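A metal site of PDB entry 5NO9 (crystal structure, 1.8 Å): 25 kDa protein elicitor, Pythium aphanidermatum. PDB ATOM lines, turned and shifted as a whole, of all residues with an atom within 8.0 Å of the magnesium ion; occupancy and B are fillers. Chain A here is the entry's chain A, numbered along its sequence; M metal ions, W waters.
The side-chain hydroxyl (OG) of Ser 126 lies within hydrogen-bond range of the side-chain carboxylate (OE1) of Glu 106, 2.6 Å away.
O of Glu 106 sits at hydrogen-bond distance from N of Trp 88.
N of His 101 sits at hydrogen-bond distance from O of Asp 93 (2.8 Å).
OH of Tyr 151 lies close to OD2 of Asp 104 (2.6 Å).
The backbone NH (N) of Asp 104 sits at hydrogen-bond distance from the backbone carbonyl oxygen (O) of Met 90 (2.8 Å).
The magnesium ion is bound by water W1 (2.1 Å), the backbone carbonyl oxygen (O) of His 159 (2.1 Å), the side-chain carboxylate (OE2) of Glu 106 (2.2 Å), the side-chain carboxylate (OD2) of Asp 93 (2.2 Å), the side-chain carboxylate (OD2) of Asp 104 (2.5 Å) and the side-chain carboxylate (OD1) of Asp 104 (2.5 Å).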
ATOM      1  N   TRP A  88      13.325  10.373  -3.190  1.00  0.00           N
ATOM      2  CA  TRP A  88      12.495  11.443  -3.727  1.00  0.00           C
ATOM      3  C   TRP A  88      13.055  12.785  -3.307  1.00  0.00           C
ATOM      4  O   TRP A  88      13.533  12.942  -2.188  1.00  0.00           O
ATOM      5  CB  TRP A  88      11.039  11.356  -3.258  1.00  0.00           C
ATOM      6  CG  TRP A  88      10.335  10.115  -3.701  1.00  0.00           C
ATOM      7  CD1 TRP A  88       9.580   9.945  -4.838  1.00  0.00           C
ATOM      8  CD2 TRP A  88      10.301   8.855  -3.006  1.00  0.00           C
ATOM      9  NE1 TRP A  88       9.100   8.665  -4.891  1.00  0.00           N
ATOM     10  CE2 TRP A  88       9.512   7.977  -3.780  1.00  0.00           C
ATOM     11  CE3 TRP A  88      10.858   8.398  -1.809  1.00  0.00           C
ATOM     12  CZ2 TRP A  88       9.269   6.659  -3.394  1.00  0.00           C
ATOM     13  CZ3 TRP A  88      10.616   7.081  -1.423  1.00  0.00           C
ATOM     14  CH2 TRP A  88       9.823   6.226  -2.214  1.00  0.00           C
ATOM     15  N   MET A  90      11.816  16.729  -2.795  1.00  0.00           N
ATOM     16  CA  MET A  90      10.719  17.703  -2.743  1.00  0.00           C
ATOM     17  C   MET A  90      11.264  19.121  -2.682  1.00  0.00           C
ATOM     18  O   MET A  90      12.306  19.355  -2.061  1.00  0.00           O
ATOM     19  CB  MET A  90       9.805  17.469  -1.536  1.00  0.00           C
ATOM     20  CG  MET A  90       8.791  16.355  -1.718  1.00  0.00           C
ATOM     21  SD  MET A  90       9.585  14.729  -1.813  1.00  0.00           S
ATOM     22  CE  MET A  90       8.143  13.681  -1.570  1.00  0.00           C
ATOM     23  N   LYS A  92      10.589  21.699  -1.003  1.00  0.00           N
ATOM     24  CA  LYS A  92      10.758  22.216   0.350  1.00  0.00           C
ATOM     25  C   LYS A  92      10.224  21.200   1.341  1.00  0.00           C
ATOM     26  O   LYS A  92       9.449  20.298   0.987  1.00  0.00           O
ATOM     27  CB  LYS A  92      10.041  23.573   0.528  1.00  0.00           C
ATOM     28  CG  LYS A  92       8.530  23.481   0.324  1.00  0.00           C
ATOM     29  CD  LYS A  92       7.852  24.814   0.595  1.00  0.00           C
ATOM     30  CE  LYS A  92       6.345  24.700   0.407  1.00  0.00           C
ATOM     31  NZ  LYS A  92       5.650  26.012   0.691  1.00  0.00           N
ATOM     32  N   ASP A  93      10.647  21.354   2.591  1.00  0.00           N
ATOM     33  CA  ASP A  93      10.143  20.581   3.734  1.00  0.00           C
ATOM     34  C   ASP A  93       9.679  21.625   4.749  1.00  0.00           C
ATOM     35  O   ASP A  93      10.463  22.063   5.594  1.00  0.00           O
ATOM     36  CB  ASP A  93      11.235  19.666   4.311  1.00  0.00           C
ATOM     37  CG  ASP A  93      10.705  18.732   5.392  1.00  0.00           C
ATOM     38  OD1 ASP A  93       9.612  18.990   5.926  1.00  0.00           O
ATOM     39  OD2 ASP A  93      11.400  17.737   5.707  1.00  0.00           O
ATOM     40  N   SER A  94       8.418  22.020   4.648  1.00  0.00           N
ATOM     41  CA  SER A  94       7.872  23.123   5.443  1.00  0.00           C
ATOM     42  C   SER A  94       6.554  22.693   6.064  1.00  0.00           C
ATOM     43  O   SER A  94       5.506  22.733   5.400  1.00  0.00           O
ATOM     44  CB  SER A  94       7.686  24.362   4.583  1.00  0.00           C
ATOM     45  OG  SER A  94       7.447  25.518   5.359  1.00  0.00           O
ATOM     46  N   HIS A 101      12.346  24.196   5.681  1.00  0.00           N
ATOM     47  CA  HIS A 101      13.516  24.605   4.926  1.00  0.00           C
ATOM     48  C   HIS A 101      13.349  24.305   3.448  1.00  0.00           C
ATOM     49  O   HIS A 101      12.526  23.483   3.033  1.00  0.00           O
ATOM     50  CB  HIS A 101      14.805  23.954   5.450  1.00  0.00           C
ATOM     51  CG  HIS A 101      14.766  22.453   5.494  1.00  0.00           C
ATOM     52  ND1 HIS A 101      14.847  21.668   4.362  1.00  0.00           N
ATOM     53  CD2 HIS A 101      14.695  21.600   6.539  1.00  0.00           C
ATOM     54  CE1 HIS A 101      14.812  20.393   4.714  1.00  0.00           C
ATOM     55  NE2 HIS A 101      14.717  20.328   6.029  1.00  0.00           N
ATOM     56  N   HIS A 103      14.320  22.619   0.049  1.00  0.00           N
ATOM     57  CA  HIS A 103      14.788  21.291  -0.380  1.00  0.00           C
ATOM     58  C   HIS A 103      14.380  20.201   0.601  1.00  0.00           C
ATOM     59  O   HIS A 103      14.320  20.428   1.815  1.00  0.00           O
ATOM     60  CB  HIS A 103      16.311  21.235  -0.548  1.00  0.00           C
ATOM     61  CG  HIS A 103      16.868  22.242  -1.494  1.00  0.00           C
ATOM     62  ND1 HIS A 103      16.439  22.369  -2.804  1.00  0.00           N
ATOM     63  CD2 HIS A 103      17.837  23.181  -1.329  1.00  0.00           C
ATOM     64  CE1 HIS A 103      17.119  23.328  -3.400  1.00  0.00           C
ATOM     65  NE2 HIS A 103      17.963  23.851  -2.522  1.00  0.00           N
ATOM     66  N   ASP A 104      14.164  18.999   0.069  1.00  0.00           N
ATOM     67  CA  ASP A 104      13.968  17.819   0.900  1.00  0.00           C
ATOM     68  C   ASP A 104      14.465  16.615   0.109  1.00  0.00           C
ATOM     69  O   ASP A 104      14.147  16.483  -1.073  1.00  0.00           O
ATOM     70  CB  ASP A 104      12.495  17.648   1.279  1.00  0.00           C
ATOM     71  CG  ASP A 104      12.298  16.786   2.513  1.00  0.00           C
ATOM     72  OD1 ASP A 104      13.292  16.533   3.209  1.00  0.00           O
ATOM     73  OD2 ASP A 104      11.155  16.367   2.777  1.00  0.00           O
ATOM     74  N   TRP A 105      15.255  15.766   0.758  1.00  0.00           N
ATOM     75  CA  TRP A 105      15.676  14.508   0.155  1.00  0.00           C
ATOM     76  C   TRP A 105      15.306  13.400   1.115  1.00  0.00           C
ATOM     77  O   TRP A 105      15.687  13.449   2.300  1.00  0.00           O
ATOM     78  CB  TRP A 105      17.183  14.503  -0.123  1.00  0.00           C
ATOM     79  CG  TRP A 105      17.619  15.156  -1.397  1.00  0.00           C
ATOM     80  CD1 TRP A 105      18.281  16.354  -1.526  1.00  0.00           C
ATOM     81  CD2 TRP A 105      17.503  14.623  -2.722  1.00  0.00           C
ATOM     82  NE1 TRP A 105      18.556  16.603  -2.853  1.00  0.00           N
ATOM     83  CE2 TRP A 105      18.085  15.557  -3.603  1.00  0.00           C
ATOM     84  CE3 TRP A 105      16.945  13.451  -3.247  1.00  0.00           C
ATOM     85  CZ2 TRP A 105      18.142  15.348  -4.989  1.00  0.00           C
ATOM     86  CZ3 TRP A 105      17.001  13.248  -4.624  1.00  0.00           C
ATOM     87  CH2 TRP A 105      17.597  14.190  -5.473  1.00  0.00           C
ATOM     88  N   GLU A 106      14.572  12.406   0.621  1.00  0.00           N
ATOM     89  CA  GLU A 106      14.162  11.270   1.426  1.00  0.00           C
ATOM     90  C   GLU A 106      14.475  10.004   0.648  1.00  0.00           C
ATOM     91  O   GLU A 106      14.572  10.015  -0.582  1.00  0.00           O
ATOM     92  CB  GLU A 106      12.656  11.316   1.750  1.00  0.00           C
ATOM     93  CG  GLU A 106      12.214  12.582   2.455  1.00  0.00           C
ATOM     94  CD  GLU A 106      12.708  12.651   3.892  1.00  0.00           C
ATOM     95  OE1 GLU A 106      13.195  11.628   4.413  1.00  0.00           O
ATOM     96  OE2 GLU A 106      12.592  13.738   4.496  1.00  0.00           O
ATOM     97  N   SER A 126      13.789   6.631   5.443  1.00  0.00           N
ATOM     98  CA  SER A 126      14.444   7.775   6.069  1.00  0.00           C
ATOM     99  C   SER A 126      13.462   8.550   6.939  1.00  0.00           C
ATOM    100  O   SER A 126      12.298   8.757   6.575  1.00  0.00           O
ATOM    101  CB  SER A 126      15.072   8.683   5.016  1.00  0.00           C
ATOM    102  OG  SER A 126      14.101   9.198   4.129  1.00  0.00           O
ATOM    103  N   ALA A 127      13.927   8.985   8.110  1.00  0.00           N
ATOM    104  CA  ALA A 127      13.134   9.793   9.024  1.00  0.00           C
ATOM    105  C   ALA A 127      14.067  10.621   9.882  1.00  0.00           C
ATOM    106  O   ALA A 127      15.099  10.107  10.348  1.00  0.00           O
ATOM    107  CB  ALA A 127      12.235   8.916   9.896  1.00  0.00           C
ATOM    108  N   HIS A 128      13.721  11.887  10.073  1.00  0.00           N
ATOM    109  CA  HIS A 128      14.445  12.872  10.901  1.00  0.00           C
ATOM    110  C   HIS A 128      15.901  12.521  11.246  1.00  0.00           C
ATOM    111  O   HIS A 128      16.189  11.996  12.318  1.00  0.00           O
ATOM    112  CB  HIS A 128      13.683  13.104  12.203  1.00  0.00           C
ATOM    113  CG  HIS A 128      12.225  13.324  12.009  1.00  0.00           C
ATOM    114  ND1 HIS A 128      11.258  12.608  12.678  1.00  0.00           N
ATOM    115  CD2 HIS A 128      11.560  14.188  11.203  1.00  0.00           C
ATOM    116  CE1 HIS A 128      10.064  13.021  12.315  1.00  0.00           C
ATOM    117  NE2 HIS A 128      10.213  13.978  11.414  1.00  0.00           N
ATOM    118  N   TYR A 151       4.695   9.721   2.853  1.00  0.00           N
ATOM    119  CA  TYR A 151       5.432  10.969   3.038  1.00  0.00           C
ATOM    120  C   TYR A 151       4.519  11.895   3.823  1.00  0.00           C
ATOM    121  O   TYR A 151       3.457  12.276   3.336  1.00  0.00           O
ATOM    122  CB  TYR A 151       5.799  11.600   1.700  1.00  0.00           C
ATOM    123  CG  TYR A 151       6.577  12.896   1.783  1.00  0.00           C
ATOM    124  CD1 TYR A 151       7.915  12.913   2.167  1.00  0.00           C
ATOM    125  CD2 TYR A 151       5.984  14.111   1.448  1.00  0.00           C
ATOM    126  CE1 TYR A 151       8.631  14.100   2.221  1.00  0.00           C
ATOM    127  CE2 TYR A 151       6.678  15.301   1.498  1.00  0.00           C
ATOM    128  CZ  TYR A 151       8.005  15.293   1.875  1.00  0.00           C
ATOM    129  OH  TYR A 151       8.722  16.475   1.921  1.00  0.00           O
ATOM    130  N   LYS A 152       4.946  12.259   5.038  1.00  0.00           N
ATOM    131  CA  LYS A 152       4.049  12.941   5.957  1.00  0.00           C
ATOM    132  C   LYS A 152       4.856  13.673   7.003  1.00  0.00           C
ATOM    133  O   LYS A 152       5.930  13.207   7.416  1.00  0.00           O
ATOM    134  CB  LYS A 152       3.082  11.938   6.616  1.00  0.00           C
ATOM    135  CG  LYS A 152       2.100  12.531   7.600  1.00  0.00           C
ATOM    136  CD  LYS A 152       1.406  11.428   8.403  1.00  0.00           C
ATOM    137  CE  LYS A 152       0.406  12.000   9.399  1.00  0.00           C
ATOM    138  NZ  LYS A 152      -0.161  10.963  10.304  1.00  0.00           N
ATOM    139  N   SER A 153       4.369  14.841   7.407  1.00  0.00           N
ATOM    140  CA  SER A 153       4.891  15.564   8.554  1.00  0.00           C
ATOM    141  C   SER A 153       3.897  15.477   9.689  1.00  0.00           C
ATOM    142  O   SER A 153       2.685  15.588   9.483  1.00  0.00           O
ATOM    143  CB  SER A 153       5.160  17.038   8.222  1.00  0.00           C
ATOM    144  OG  SER A 153       5.341  17.798   9.409  1.00  0.00           O
ATOM    145  N   ASP A 158       9.104  17.576  10.837  1.00  0.00           N
ATOM    146  CA  ASP A 158       9.494  17.621   9.417  1.00  0.00           C
ATOM    147  C   ASP A 158       8.836  16.483   8.652  1.00  0.00           C
ATOM    148  O   ASP A 158       8.533  15.435   9.224  1.00  0.00           O
ATOM    149  CB  ASP A 158      11.022  17.531   9.273  1.00  0.00           C
ATOM    150  CG  ASP A 158      11.710  18.864   9.528  1.00  0.00           C
ATOM    151  OD1 ASP A 158      11.044  19.920   9.479  1.00  0.00           O
ATOM    152  OD2 ASP A 158      12.944  18.849   9.754  1.00  0.00           O
ATOM    153  N   HIS A 159       8.611  16.681   7.349  1.00  0.00           N
ATOM    154  CA  HIS A 159       8.064  15.612   6.522  1.00  0.00           C
ATOM    155  C   HIS A 159       9.065  14.467   6.433  1.00  0.00           C
ATOM    156  O   HIS A 159      10.232  14.680   6.106  1.00  0.00           O
ATOM    157  CB  HIS A 159       7.728  16.115   5.120  1.00  0.00           C
ATOM    158  CG  HIS A 159       6.669  17.165   5.086  1.00  0.00           C
ATOM    159  ND1 HIS A 159       6.922  18.497   5.374  1.00  0.00           N
ATOM    160  CD2 HIS A 159       5.353  17.104   4.783  1.00  0.00           C
ATOM    161  CE1 HIS A 159       5.808  19.194   5.261  1.00  0.00           C
ATOM    162  NE2 HIS A 159       4.835  18.368   4.909  1.00  0.00           N
ATOM    163  N   GLU A 160       8.591  13.256   6.699  1.00  0.00           N
ATOM    164  CA  GLU A 160       9.440  12.086   6.807  1.00  0.00           C
ATOM    165  C   GLU A 160       8.793  10.932   6.055  1.00  0.00           C
ATOM    166  O   GLU A 160       7.583  10.927   5.808  1.00  0.00           O
ATOM    167  CB  GLU A 160       9.645  11.703   8.261  1.00  0.00           C
ATOM    168  CG  GLU A 160       8.377  11.129   8.864  1.00  0.00           C
ATOM    169  CD  GLU A 160       8.344  11.183  10.371  1.00  0.00           C
ATOM    170  OE1 GLU A 160       9.087  10.414  11.010  1.00  0.00           O
ATOM    171  OE2 GLU A 160       7.554  12.000  10.914  1.00  0.00           O
ATOM    172  N   LEU A 161       9.609   9.954   5.699  1.00  0.00           N
ATOM    173  CA  LEU A 161       9.036   8.739   5.153  1.00  0.00           C
ATOM    174  C   LEU A 161       8.614   7.797   6.286  1.00  0.00           C
ATOM    175  O   LEU A 161       9.019   7.925   7.443  1.00  0.00           O
ATOM    176  CB  LEU A 161      10.036   8.038   4.234  1.00  0.00           C
ATOM    177  CG  LEU A 161      10.411   8.804   2.962  1.00  0.00           C
ATOM    178  CD1 LEU A 161      11.350   7.988   2.104  1.00  0.00           C
ATOM    179  CD2 LEU A 161       9.161   9.235   2.179  1.00  0.00           C
ATOM    180  N   ALA A 195      18.999  19.677   3.367  1.00  0.00           N
ATOM    181  CA  ALA A 195      18.761  18.379   2.741  1.00  0.00           C
ATOM    182  C   ALA A 195      20.056  17.819   2.155  1.00  0.00           C
ATOM    183  O   ALA A 195      20.962  18.571   1.772  1.00  0.00           O
ATOM    184  CB  ALA A 195      17.698  18.496   1.644  1.00  0.00           C
HETATM  185 MG    MG M   1      11.850  15.666   5.119  1.00  0.00          MG
HETATM  186  O   HOH W   1      13.577  15.507   6.332  1.00  0.00           O
